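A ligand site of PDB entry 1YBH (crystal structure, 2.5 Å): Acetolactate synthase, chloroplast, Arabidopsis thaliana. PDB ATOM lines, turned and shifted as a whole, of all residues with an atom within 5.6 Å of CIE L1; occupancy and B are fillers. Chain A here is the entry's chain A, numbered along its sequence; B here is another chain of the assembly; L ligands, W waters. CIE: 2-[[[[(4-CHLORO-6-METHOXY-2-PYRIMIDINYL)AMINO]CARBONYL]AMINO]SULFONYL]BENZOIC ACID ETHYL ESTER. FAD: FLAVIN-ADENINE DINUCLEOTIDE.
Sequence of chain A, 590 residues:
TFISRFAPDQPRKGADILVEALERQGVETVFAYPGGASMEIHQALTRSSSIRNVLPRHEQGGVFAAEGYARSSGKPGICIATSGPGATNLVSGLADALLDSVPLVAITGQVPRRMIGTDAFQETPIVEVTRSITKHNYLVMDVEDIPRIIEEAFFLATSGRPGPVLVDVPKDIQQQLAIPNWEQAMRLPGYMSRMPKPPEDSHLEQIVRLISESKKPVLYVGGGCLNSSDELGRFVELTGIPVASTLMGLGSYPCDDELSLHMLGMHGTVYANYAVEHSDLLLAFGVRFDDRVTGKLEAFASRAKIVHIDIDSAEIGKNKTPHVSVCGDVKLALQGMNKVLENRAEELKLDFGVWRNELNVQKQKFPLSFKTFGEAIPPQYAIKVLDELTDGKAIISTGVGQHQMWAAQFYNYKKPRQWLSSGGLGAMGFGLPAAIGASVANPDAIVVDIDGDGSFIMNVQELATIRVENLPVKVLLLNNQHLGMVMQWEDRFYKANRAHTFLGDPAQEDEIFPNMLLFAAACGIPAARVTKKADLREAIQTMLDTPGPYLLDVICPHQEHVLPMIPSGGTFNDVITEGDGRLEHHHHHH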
ATOM      1  N   MET A 266      -2.569  12.809  10.272  1.00  0.00           N
ATOM      2  CA  MET A 266      -3.885  13.422  10.370  1.00  0.00           C
ATOM      3  C   MET A 266      -5.016  12.430  10.585  1.00  0.00           C
ATOM      4  O   MET A 266      -5.863  12.626  11.465  1.00  0.00           O
ATOM      5  CB  MET A 266      -4.150  14.250   9.112  1.00  0.00           C
ATOM      6  CG  MET A 266      -5.496  14.943   9.086  1.00  0.00           C
ATOM      7  SD  MET A 266      -5.634  16.083   7.707  1.00  0.00           S
ATOM      8  CE  MET A 266      -4.802  17.522   8.402  1.00  0.00           C
ATOM      9  N   HIS A 267      -5.037  11.367   9.786  1.00  0.00           N
ATOM     10  CA  HIS A 267      -6.056  10.353   9.913  1.00  0.00           C
ATOM     11  C   HIS A 267      -5.437   9.034  10.351  1.00  0.00           C
ATOM     12  O   HIS A 267      -5.935   7.952  10.017  1.00  0.00           O
ATOM     13  CB  HIS A 267      -6.802  10.178   8.595  1.00  0.00           C
ATOM     14  CG  HIS A 267      -7.639  11.353   8.228  1.00  0.00           C
ATOM     15  ND1 HIS A 267      -8.612  11.865   9.063  1.00  0.00           N
ATOM     16  CD2 HIS A 267      -7.636  12.141   7.124  1.00  0.00           C
ATOM     17  CE1 HIS A 267      -9.179  12.915   8.481  1.00  0.00           C
ATOM     18  NE2 HIS A 267      -8.604  13.102   7.304  1.00  0.00           N
ATOM     19  N   ASP A 291       3.587  17.592   6.275  1.00  0.00           N
ATOM     20  CA  ASP A 291       2.714  18.268   7.226  1.00  0.00           C
ATOM     21  C   ASP A 291       1.513  17.398   7.612  1.00  0.00           C
ATOM     22  O   ASP A 291       0.956  17.546   8.694  1.00  0.00           O
ATOM     23  CB  ASP A 291       2.233  19.620   6.652  1.00  0.00           C
ATOM     24  CG  ASP A 291       1.531  19.483   5.306  1.00  0.00           C
ATOM     25  OD1 ASP A 291       2.206  19.601   4.249  1.00  0.00           O
ATOM     26  OD2 ASP A 291       0.304  19.246   5.295  1.00  0.00           O
ATOM     27  N   ARG A 292       1.128  16.497   6.717  1.00  0.00           N
ATOM     28  CA  ARG A 292       0.008  15.598   6.985  1.00  0.00           C
ATOM     29  C   ARG A 292       0.279  14.690   8.168  1.00  0.00           C
ATOM     30  O   ARG A 292      -0.634  14.396   8.943  1.00  0.00           O
ATOM     31  CB  ARG A 292      -0.301  14.751   5.756  1.00  0.00           C
ATOM     32  CG  ARG A 292      -1.484  15.242   4.955  1.00  0.00           C
ATOM     33  CD  ARG A 292      -1.482  16.747   4.922  1.00  0.00           C
ATOM     34  NE  ARG A 292      -2.836  17.268   5.025  1.00  0.00           N
ATOM     35  CZ  ARG A 292      -3.129  18.505   5.390  1.00  0.00           C
ATOM     36  NH1 ARG A 292      -2.179  19.374   5.685  1.00  0.00           N
ATOM     37  NH2 ARG A 292      -4.407  18.876   5.438  1.00  0.00           N
ATOM     38  N   MET A 485     -14.753  14.226   1.555  1.00  0.00           N
ATOM     39  CA  MET A 485     -13.775  14.936   2.353  1.00  0.00           C
ATOM     40  C   MET A 485     -14.093  16.424   2.502  1.00  0.00           C
ATOM     41  O   MET A 485     -13.992  16.965   3.602  1.00  0.00           O
ATOM     42  CB  MET A 485     -12.375  14.745   1.765  1.00  0.00           C
ATOM     43  CG  MET A 485     -11.241  15.235   2.656  1.00  0.00           C
ATOM     44  SD  MET A 485     -11.253  14.467   4.288  1.00  0.00           S
ATOM     45  CE  MET A 485     -10.531  12.863   3.908  1.00  0.00           C
ATOM     46  N   VAL A 486     -14.482  17.087   1.416  1.00  0.00           N
ATOM     47  CA  VAL A 486     -14.800  18.510   1.490  1.00  0.00           C
ATOM     48  C   VAL A 486     -16.026  18.705   2.363  1.00  0.00           C
ATOM     49  O   VAL A 486     -16.138  19.678   3.116  1.00  0.00           O
ATOM     50  CB  VAL A 486     -15.091  19.111   0.114  1.00  0.00           C
ATOM     51  CG1 VAL A 486     -15.380  20.599   0.229  1.00  0.00           C
ATOM     52  CG2 VAL A 486     -13.917  18.887  -0.796  1.00  0.00           C
ATOM     53  N   TRP A 489     -15.229  18.539   6.076  1.00  0.00           N
ATOM     54  CA  TRP A 489     -14.677  19.803   6.539  1.00  0.00           C
ATOM     55  C   TRP A 489     -15.761  20.863   6.661  1.00  0.00           C
ATOM     56  O   TRP A 489     -15.692  21.740   7.526  1.00  0.00           O
ATOM     57  CB  TRP A 489     -13.542  20.254   5.603  1.00  0.00           C
ATOM     58  CG  TRP A 489     -12.227  19.588   5.912  1.00  0.00           C
ATOM     59  CD1 TRP A 489     -11.975  18.244   5.933  1.00  0.00           C
ATOM     60  CD2 TRP A 489     -11.015  20.233   6.347  1.00  0.00           C
ATOM     61  NE1 TRP A 489     -10.687  18.015   6.359  1.00  0.00           N
ATOM     62  CE2 TRP A 489     -10.076  19.215   6.616  1.00  0.00           C
ATOM     63  CE3 TRP A 489     -10.648  21.572   6.528  1.00  0.00           C
ATOM     64  CZ2 TRP A 489      -8.781  19.493   7.069  1.00  0.00           C
ATOM     65  CZ3 TRP A 489      -9.357  21.841   6.976  1.00  0.00           C
ATOM     66  CH2 TRP A 489      -8.444  20.812   7.247  1.00  0.00           C
ATOM     67  N   SER A 568      -5.251  20.388  10.812  1.00  0.00           N
ATOM     68  CA  SER A 568      -3.996  20.914  10.284  1.00  0.00           C
ATOM     69  C   SER A 568      -3.206  21.753  11.273  1.00  0.00           C
ATOM     70  O   SER A 568      -3.780  22.632  11.916  1.00  0.00           O
ATOM     71  CB  SER A 568      -4.249  21.754   9.041  1.00  0.00           C
ATOM     72  OG  SER A 568      -4.688  20.947   7.965  1.00  0.00           O
ATOM     73  N   GLY A 569      -1.908  21.481  11.364  1.00  0.00           N
ATOM     74  CA  GLY A 569      -1.058  22.238  12.270  1.00  0.00           C
ATOM     75  C   GLY A 569      -1.392  21.951  13.719  1.00  0.00           C
ATOM     76  O   GLY A 569      -1.012  22.705  14.624  1.00  0.00           O
ATOM     77  N   GLY B  35     -12.377  22.365  -3.496  1.00  0.00           N
ATOM     78  CA  GLY B  35     -11.256  21.592  -3.005  1.00  0.00           C
ATOM     79  C   GLY B  35     -10.826  22.228  -1.690  1.00  0.00           C
ATOM     80  O   GLY B  35     -11.231  23.339  -1.375  1.00  0.00           O
ATOM     81  N   GLY B  36      -9.996  21.527  -0.922  1.00  0.00           N
ATOM     82  CA  GLY B  36      -9.552  22.036   0.360  1.00  0.00           C
ATOM     83  C   GLY B  36      -8.980  23.449   0.395  1.00  0.00           C
ATOM     84  O   GLY B  36      -9.318  24.250   1.266  1.00  0.00           O
ATOM     85  N   ALA B  37      -8.118  23.756  -0.573  1.00  0.00           N
ATOM     86  CA  ALA B  37      -7.487  25.075  -0.616  1.00  0.00           C
ATOM     87  C   ALA B  37      -8.392  26.187  -1.120  1.00  0.00           C
ATOM     88  O   ALA B  37      -8.028  27.359  -1.027  1.00  0.00           O
ATOM     89  CB  ALA B  37      -6.215  25.007  -1.476  1.00  0.00           C
ATOM     90  N   MET B  39     -11.962  26.105  -0.356  1.00  0.00           N
ATOM     91  CA  MET B  39     -13.216  26.041   0.393  1.00  0.00           C
ATOM     92  C   MET B  39     -13.761  27.402   0.809  1.00  0.00           C
ATOM     93  O   MET B  39     -14.952  27.657   0.708  1.00  0.00           O
ATOM     94  CB  MET B  39     -13.061  25.178   1.642  1.00  0.00           C
ATOM     95  CG  MET B  39     -13.073  23.697   1.352  1.00  0.00           C
ATOM     96  SD  MET B  39     -12.985  22.789   2.878  1.00  0.00           S
ATOM     97  CE  MET B  39     -14.722  22.909   3.402  1.00  0.00           C
ATOM     98  N   THR B  82      -9.239  24.382  -6.956  1.00  0.00           N
ATOM     99  CA  THR B  82      -8.488  24.300  -5.723  1.00  0.00           C
ATOM    100  C   THR B  82      -7.012  24.182  -6.098  1.00  0.00           C
ATOM    101  O   THR B  82      -6.659  24.221  -7.277  1.00  0.00           O
ATOM    102  CB  THR B  82      -8.937  23.088  -4.885  1.00  0.00           C
ATOM    103  OG1 THR B  82      -8.371  23.179  -3.570  1.00  0.00           O
ATOM    104  CG2 THR B  82      -8.482  21.806  -5.540  1.00  0.00           C
ATOM    105  N   SER B  83      -6.149  24.033  -5.102  1.00  0.00           N
ATOM    106  CA  SER B  83      -4.727  23.936  -5.348  1.00  0.00           C
ATOM    107  C   SER B  83      -4.307  22.601  -5.950  1.00  0.00           C
ATOM    108  O   SER B  83      -5.114  21.701  -6.154  1.00  0.00           O
ATOM    109  CB  SER B  83      -3.958  24.165  -4.042  1.00  0.00           C
ATOM    110  OG  SER B  83      -4.164  23.097  -3.136  1.00  0.00           O
ATOM    111  N   GLN B 110      -4.536  28.147  -3.223  1.00  0.00           N
ATOM    112  CA  GLN B 110      -3.148  27.738  -3.038  1.00  0.00           C
ATOM    113  C   GLN B 110      -2.961  27.483  -1.550  1.00  0.00           C
ATOM    114  O   GLN B 110      -3.748  27.956  -0.740  1.00  0.00           O
ATOM    115  CB  GLN B 110      -2.231  28.874  -3.519  1.00  0.00           C
ATOM    116  CG  GLN B 110      -0.734  28.619  -3.350  1.00  0.00           C
ATOM    117  CD  GLN B 110      -0.265  27.312  -3.964  1.00  0.00           C
ATOM    118  OE1 GLN B 110      -0.454  26.241  -3.383  1.00  0.00           O
ATOM    119  NE2 GLN B 110       0.327  27.386  -5.155  1.00  0.00           N
ATOM    120  N   VAL B 111      -1.934  26.724  -1.201  1.00  0.00           N
ATOM    121  CA  VAL B 111      -1.678  26.442   0.211  1.00  0.00           C
ATOM    122  C   VAL B 111      -1.332  27.771   0.892  1.00  0.00           C
ATOM    123  O   VAL B 111      -1.075  28.775   0.211  1.00  0.00           O
ATOM    124  CB  VAL B 111      -0.505  25.455   0.371  1.00  0.00           C
ATOM    125  CG1 VAL B 111      -0.808  24.164  -0.338  1.00  0.00           C
ATOM    126  CG2 VAL B 111       0.770  26.072  -0.194  1.00  0.00           C
ATOM    127  N   PRO B 112      -1.343  27.806   2.233  1.00  0.00           N
ATOM    128  CA  PRO B 112      -1.014  29.052   2.931  1.00  0.00           C
ATOM    129  C   PRO B 112       0.378  29.532   2.511  1.00  0.00           C
ATOM    130  O   PRO B 112       1.247  28.723   2.212  1.00  0.00           O
ATOM    131  CB  PRO B 112      -1.051  28.656   4.408  1.00  0.00           C
ATOM    132  CG  PRO B 112      -2.005  27.474   4.423  1.00  0.00           C
ATOM    133  CD  PRO B 112      -1.604  26.715   3.180  1.00  0.00           C
ATOM    134  N   MET B 115       3.549  28.015   3.735  1.00  0.00           N
ATOM    135  CA  MET B 115       3.732  26.642   3.262  1.00  0.00           C
ATOM    136  C   MET B 115       4.274  26.546   1.852  1.00  0.00           C
ATOM    137  O   MET B 115       4.748  25.489   1.437  1.00  0.00           O
ATOM    138  CB  MET B 115       2.397  25.880   3.308  1.00  0.00           C
ATOM    139  CG  MET B 115       1.730  25.794   4.675  1.00  0.00           C
ATOM    140  SD  MET B 115       2.839  25.119   5.913  1.00  0.00           S
ATOM    141  CE  MET B 115       3.220  23.514   5.196  1.00  0.00           C
ATOM    142  N   ALA B 120       4.368  21.175   0.239  1.00  0.00           N
ATOM    143  CA  ALA B 120       3.164  21.007   1.054  1.00  0.00           C
ATOM    144  C   ALA B 120       2.105  20.137   0.417  1.00  0.00           C
ATOM    145  O   ALA B 120       2.163  19.803  -0.769  1.00  0.00           O
ATOM    146  CB  ALA B 120       2.577  22.361   1.370  1.00  0.00           C
ATOM    147  N   PHE B 121       1.114  19.797   1.227  1.00  0.00           N
ATOM    148  CA  PHE B 121      -0.001  18.981   0.788  1.00  0.00           C
ATOM    149  C   PHE B 121      -0.739  19.693  -0.345  1.00  0.00           C
ATOM    150  O   PHE B 121      -1.132  20.852  -0.213  1.00  0.00           O
ATOM    151  CB  PHE B 121      -0.947  18.741   1.959  1.00  0.00           C
ATOM    152  CG  PHE B 121      -2.165  17.944   1.603  1.00  0.00           C
ATOM    153  CD1 PHE B 121      -2.034  16.703   0.998  1.00  0.00           C
ATOM    154  CD2 PHE B 121      -3.435  18.427   1.887  1.00  0.00           C
ATOM    155  CE1 PHE B 121      -3.152  15.950   0.671  1.00  0.00           C
ATOM    156  CE2 PHE B 121      -4.559  17.671   1.574  1.00  0.00           C
ATOM    157  CZ  PHE B 121      -4.415  16.437   0.967  1.00  0.00           C
ATOM    158  N   GLN B 122      -0.931  18.987  -1.455  1.00  0.00           N
ATOM    159  CA  GLN B 122      -1.622  19.530  -2.621  1.00  0.00           C
ATOM    160  C   GLN B 122      -1.053  20.860  -3.123  1.00  0.00           C
ATOM    161  O   GLN B 122      -1.795  21.729  -3.574  1.00  0.00           O
ATOM    162  CB  GLN B 122      -3.106  19.688  -2.330  1.00  0.00           C
ATOM    163  CG  GLN B 122      -3.788  18.401  -1.958  1.00  0.00           C
ATOM    164  CD  GLN B 122      -5.231  18.355  -2.427  1.00  0.00           C
ATOM    165  OE1 GLN B 122      -6.075  19.176  -2.019  1.00  0.00           O
ATOM    166  NE2 GLN B 122      -5.541  17.392  -3.299  1.00  0.00           N
ATOM    167  N   LYS B 171      -4.489  30.132   0.873  1.00  0.00           N
ATOM    168  CA  LYS B 171      -5.595  29.895   1.783  1.00  0.00           C
ATOM    169  C   LYS B 171      -5.609  30.859   2.973  1.00  0.00           C
ATOM    170  O   LYS B 171      -6.674  31.270   3.424  1.00  0.00           O
ATOM    171  CB  LYS B 171      -5.556  28.444   2.263  1.00  0.00           C
ATOM    172  CG  LYS B 171      -6.735  28.024   3.098  1.00  0.00           C
ATOM    173  CD  LYS B 171      -6.818  26.515   3.157  1.00  0.00           C
ATOM    174  CE  LYS B 171      -7.910  26.039   4.100  1.00  0.00           C
ATOM    175  NZ  LYS B 171      -7.551  26.267   5.520  1.00  0.00           N
HETATM  176  C1  CIE L   1      -2.689  23.173   3.262  1.00  0.00           C
HETATM  177  C2  CIE L   1      -2.837  23.458   4.729  1.00  0.00           C
HETATM  178  C3  CIE L   1      -1.715  23.201   5.681  1.00  0.00           C
HETATM  179  C4  CIE L   1      -0.430  22.652   5.194  1.00  0.00           C
HETATM  180  C5  CIE L   1      -0.219  22.350   3.744  1.00  0.00           C
HETATM  181  C6  CIE L   1      -1.348  22.617   2.776  1.00  0.00           C
HETATM  182  C7  CIE L   1      -3.768  23.418   2.313  1.00  0.00           C
HETATM  183  O7  CIE L   1      -4.093  24.633   2.005  1.00  0.00           O
HETATM  184  O8  CIE L   1      -4.400  22.275   1.780  1.00  0.00           O
HETATM  185  C9  CIE L   1      -5.398  22.222   0.914  1.00  0.00           C
HETATM  186  C10 CIE L   1      -5.835  20.820   0.572  1.00  0.00           C
HETATM  187  S11 CIE L   1      -4.292  24.081   5.428  1.00  0.00           S
HETATM  188  OBA CIE L   1      -4.330  23.703   6.917  1.00  0.00           O
HETATM  189  OBB CIE L   1      -4.463  25.653   5.226  1.00  0.00           O
HETATM  190  N12 CIE L   1      -5.728  23.437   4.789  1.00  0.00           N
HETATM  191  C13 CIE L   1      -5.984  22.111   4.724  1.00  0.00           C
HETATM  192  O13 CIE L   1      -5.095  21.287   5.141  1.00  0.00           O
HETATM  193  N14 CIE L   1      -7.170  21.747   4.195  1.00  0.00           N
HETATM  194  N1' CIE L   1      -6.940  19.393   4.279  1.00  0.00           N
HETATM  195  C2' CIE L   1      -7.673  20.500   3.970  1.00  0.00           C
HETATM  196  N3' CIE L   1      -8.964  20.424   3.408  1.00  0.00           N
HETATM  197  C4' CIE L   1      -9.527  19.132   3.139  1.00  0.00           C
HETATM  198 CL4' CIE L   1     -10.942  19.064   2.514  1.00  0.00          CL
HETATM  199  C5' CIE L   1      -8.786  17.864   3.445  1.00  0.00           C
HETATM  200  C6' CIE L   1      -7.394  18.142   4.059  1.00  0.00           C
HETATM  201  O7' CIE L   1      -6.533  17.141   4.414  1.00  0.00           O
HETATM  202  C8' CIE L   1      -6.721  15.774   4.302  1.00  0.00           C
HETATM  203  PA  FAD L   2       7.089   9.841   0.151  1.00  0.00           P
HETATM  204  O1A FAD L   2       7.024   8.801  -0.901  1.00  0.00           O
HETATM  205  O2A FAD L   2       6.400  11.089   0.022  1.00  0.00           O
HETATM  206  O5B FAD L   2       8.502  10.238   0.489  1.00  0.00           O
HETATM  207  C5B FAD L   2       9.524   9.179   0.584  1.00  0.00           C
HETATM  208  C4B FAD L   2      10.806   9.791   1.037  1.00  0.00           C
HETATM  209  O4B FAD L   2      11.721   8.703   1.077  1.00  0.00           O
HETATM  210  C3B FAD L   2      11.572  10.940   0.260  1.00  0.00           C
HETATM  211  O3B FAD L   2      12.131  11.959   1.059  1.00  0.00           O
HETATM  212  C2B FAD L   2      12.490  10.139  -0.598  1.00  0.00           C
HETATM  213  O2B FAD L   2      13.413  10.745  -1.405  1.00  0.00           O
HETATM  214  C1B FAD L   2      12.919   9.072   0.422  1.00  0.00           C
HETATM  215  N9A FAD L   2      13.480   7.754  -0.143  1.00  0.00           N
HETATM  216  C8A FAD L   2      13.026   7.215  -1.428  1.00  0.00           C
HETATM  217  N7A FAD L   2      13.576   6.097  -1.796  1.00  0.00           N
HETATM  218  C5A FAD L   2      14.448   5.801  -0.808  1.00  0.00           C
HETATM  219  C6A FAD L   2      15.478   4.678  -0.462  1.00  0.00           C
HETATM  220  N6A FAD L   2      15.656   3.651  -1.258  1.00  0.00           N
HETATM  221  N1A FAD L   2      16.245   4.754   0.776  1.00  0.00           N
HETATM  222  C2A FAD L   2      16.076   5.868   1.695  1.00  0.00           C
HETATM  223  N3A FAD L   2      15.183   6.913   1.475  1.00  0.00           N
HETATM  224  C4A FAD L   2      14.393   6.852   0.230  1.00  0.00           C
HETATM  225  N1  FAD L   2      -0.217  10.607   5.053  1.00  0.00           N
HETATM  226  C2  FAD L   2      -0.100  10.099   6.288  1.00  0.00           C
HETATM  227  O2  FAD L   2       0.923   9.456   6.539  1.00  0.00           O
HETATM  228  N3  FAD L   2      -1.147  10.214   7.236  1.00  0.00           N
HETATM  229  C4  FAD L   2      -2.387  10.831   6.920  1.00  0.00           C
HETATM  230  O4  FAD L   2      -3.264  11.019   7.770  1.00  0.00           O
HETATM  231  C4X FAD L   2      -2.549  11.293   5.538  1.00  0.00           C
HETATM  232  N5  FAD L   2      -3.753  11.829   5.138  1.00  0.00           N
HETATM  233  C5X FAD L   2      -3.898  12.230   3.822  1.00  0.00           C
HETATM  234  C6  FAD L   2      -5.202  12.616   3.388  1.00  0.00           C
HETATM  235  C7  FAD L   2      -5.465  12.851   2.011  1.00  0.00           C
HETATM  236  C7M FAD L   2      -6.894  13.082   1.585  1.00  0.00           C
HETATM  237  C8  FAD L   2      -4.376  12.759   1.040  1.00  0.00           C
HETATM  238  C8M FAD L   2      -4.586  12.885  -0.458  1.00  0.00           C
HETATM  239  C9  FAD L   2      -3.059  12.468   1.491  1.00  0.00           C
HETATM  240  C9A FAD L   2      -2.789  12.128   2.850  1.00  0.00           C
HETATM  241  N10 FAD L   2      -1.514  11.705   3.320  1.00  0.00           N
HETATM  242  C10 FAD L   2      -1.394  11.186   4.633  1.00  0.00           C
HETATM  243  C1' FAD L   2      -0.401  11.434   2.342  1.00  0.00           C
HETATM  244  C2' FAD L   2       0.517  12.565   2.490  1.00  0.00           C
HETATM  245  O2' FAD L   2       0.129  13.703   1.706  1.00  0.00           O
HETATM  246  C3' FAD L   2       1.970  12.298   2.069  1.00  0.00           C
HETATM  247  O3' FAD L   2       1.871  11.836   0.614  1.00  0.00           O
HETATM  248  C4' FAD L   2       2.695  11.122   2.802  1.00  0.00           C
HETATM  249  O4' FAD L   2       2.588  11.439   4.286  1.00  0.00           O
HETATM  250  C5' FAD L   2       4.108  11.089   2.391  1.00  0.00           C
HETATM  251  O5' FAD L   2       4.735   9.979   3.124  1.00  0.00           O
HETATM  252  P   FAD L   2       6.240   9.630   2.940  1.00  0.00           P
HETATM  253  O1P FAD L   2       6.986  10.858   3.303  1.00  0.00           O
HETATM  254  O2P FAD L   2       6.486   8.531   3.808  1.00  0.00           O
HETATM  255  O3P FAD L   2       6.508   9.119   1.454  1.00  0.00           O
HETATM  256  O   HOH W   1      -8.987  15.956   6.724  1.00  0.00           O
HETATM  257  O   HOH W   2      -6.617  21.787  -2.511  1.00  0.00           O
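SD of Met 266 lies close to O7' of CIE L1 (3.6 Å). OD2 of Asp 291 touches C4 of CIE L1, at 3.5 Å. Met 485 touches CIE L1. Trp 489 touches CIE L1. Gly 36 of chain B touches CIE L1. N of Ala 37 of chain B touches C9 of CIE L1, at 3.5 Å. Val 111 of chain B touches CIE L1. Pro 112 of chain B touches CIE L1 (CG to OBB, 3.2 Å). Met 115 of chain B touches CIE L1. CB of Ala 120 of chain B touches C5 of CIE L1, at 3.7 Å. Phe 121 of chain B touches CIE L1. Gln 122 of chain B touches CIE L1 (OE1 to C10, 3.1 Å). Hydrophobic or aromatic side chains that line CIE L1: Met 266, Met 485, Trp 489, Ala 37 of chain B, Val 111 of chain B, Pro 112 of chain B, Met 115 of chain B, Ala 120 of chain B and Phe 121 of chain B. Within 4 Å of CIE L1: Met 266, Asp 291, Arg 292, Met 485, Trp 489, Ser 568, Gly 36 of chain B, Ala 37 of chain B, Val 111 of chain B, Pro 112 of chain B, Met 115 of chain B, Ala 120 of chain B, Phe 121 of chain B, Gln 122 of chain B and Lys 171 of chain B. The nearest printed residue that does not touch CIE L1 is Val 486 (4.03 Å).
Water W1 lies within hydrogen-bond range of the indole nitrogen (NE1) of Trp 489 (2.7 Å), a ring nitrogen (NE2) of His 267 (2.9 Å), the side-chain sulfur (SD) of Met 266 (3.5 Å) and the side-chain sulfur (SD) of Met 485 (3.6 Å). Water W2 lies within hydrogen-bond range of the side-chain hydroxyl (OG1) of Thr 82 of chain B (2.5 Å), the side-chain amide oxygen (OE1) of Gln 122 of chain B (2.7 Å), the side-chain hydroxyl (OG) of Ser 83 of chain B (2.9 Å) and the backbone NH (N) of Ala 37 of chain B (3.1 Å).
O13 of CIE L1 lies within hydrogen-bond range of NH2 of Arg 292. The side-chain hydroxyl (OG) of Ser 568 lies within hydrogen-bond range of an oxygen (O13) of CIE L1, at 2.9 Å. The side-chain amino group (NZ) of Lys 171 of chain B is in hydrogen-bond range of an oxygen (OBB) of CIE L1, 3.2 Å away. O4 of FAD L2 lies within hydrogen-bond range of N of Met 266 (3.2 Å). The backbone NH (N) of His 267 sits at hydrogen-bond distance from an oxygen (O4) of FAD L2 (2.7 Å).
OG of Ser 568 is in hydrogen-bond range of NH2 of Arg 292, at 3.3 Å. NH1 of Arg 292 is in salt-bridge range of OD2 of Asp 291 (2.5 Å). The backbone carbonyl oxygen of Arg 292 is in hydrogen-bond range of the backbone NH of Met 266, at 2.8 Å. O of Gln 122 of chain B is in hydrogen-bond range of OG of Ser 83 of chain B (2.8 Å). The backbone NH (N) of Ala 37 of chain B is in hydrogen-bond range of the side-chain hydroxyl (OG1) of Thr 82 of chain B, 3.1 Å away. The backbone NH of Phe 121 of chain B is in hydrogen-bond range of the side-chain carboxylate of Asp 291, at 3.2 Å.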
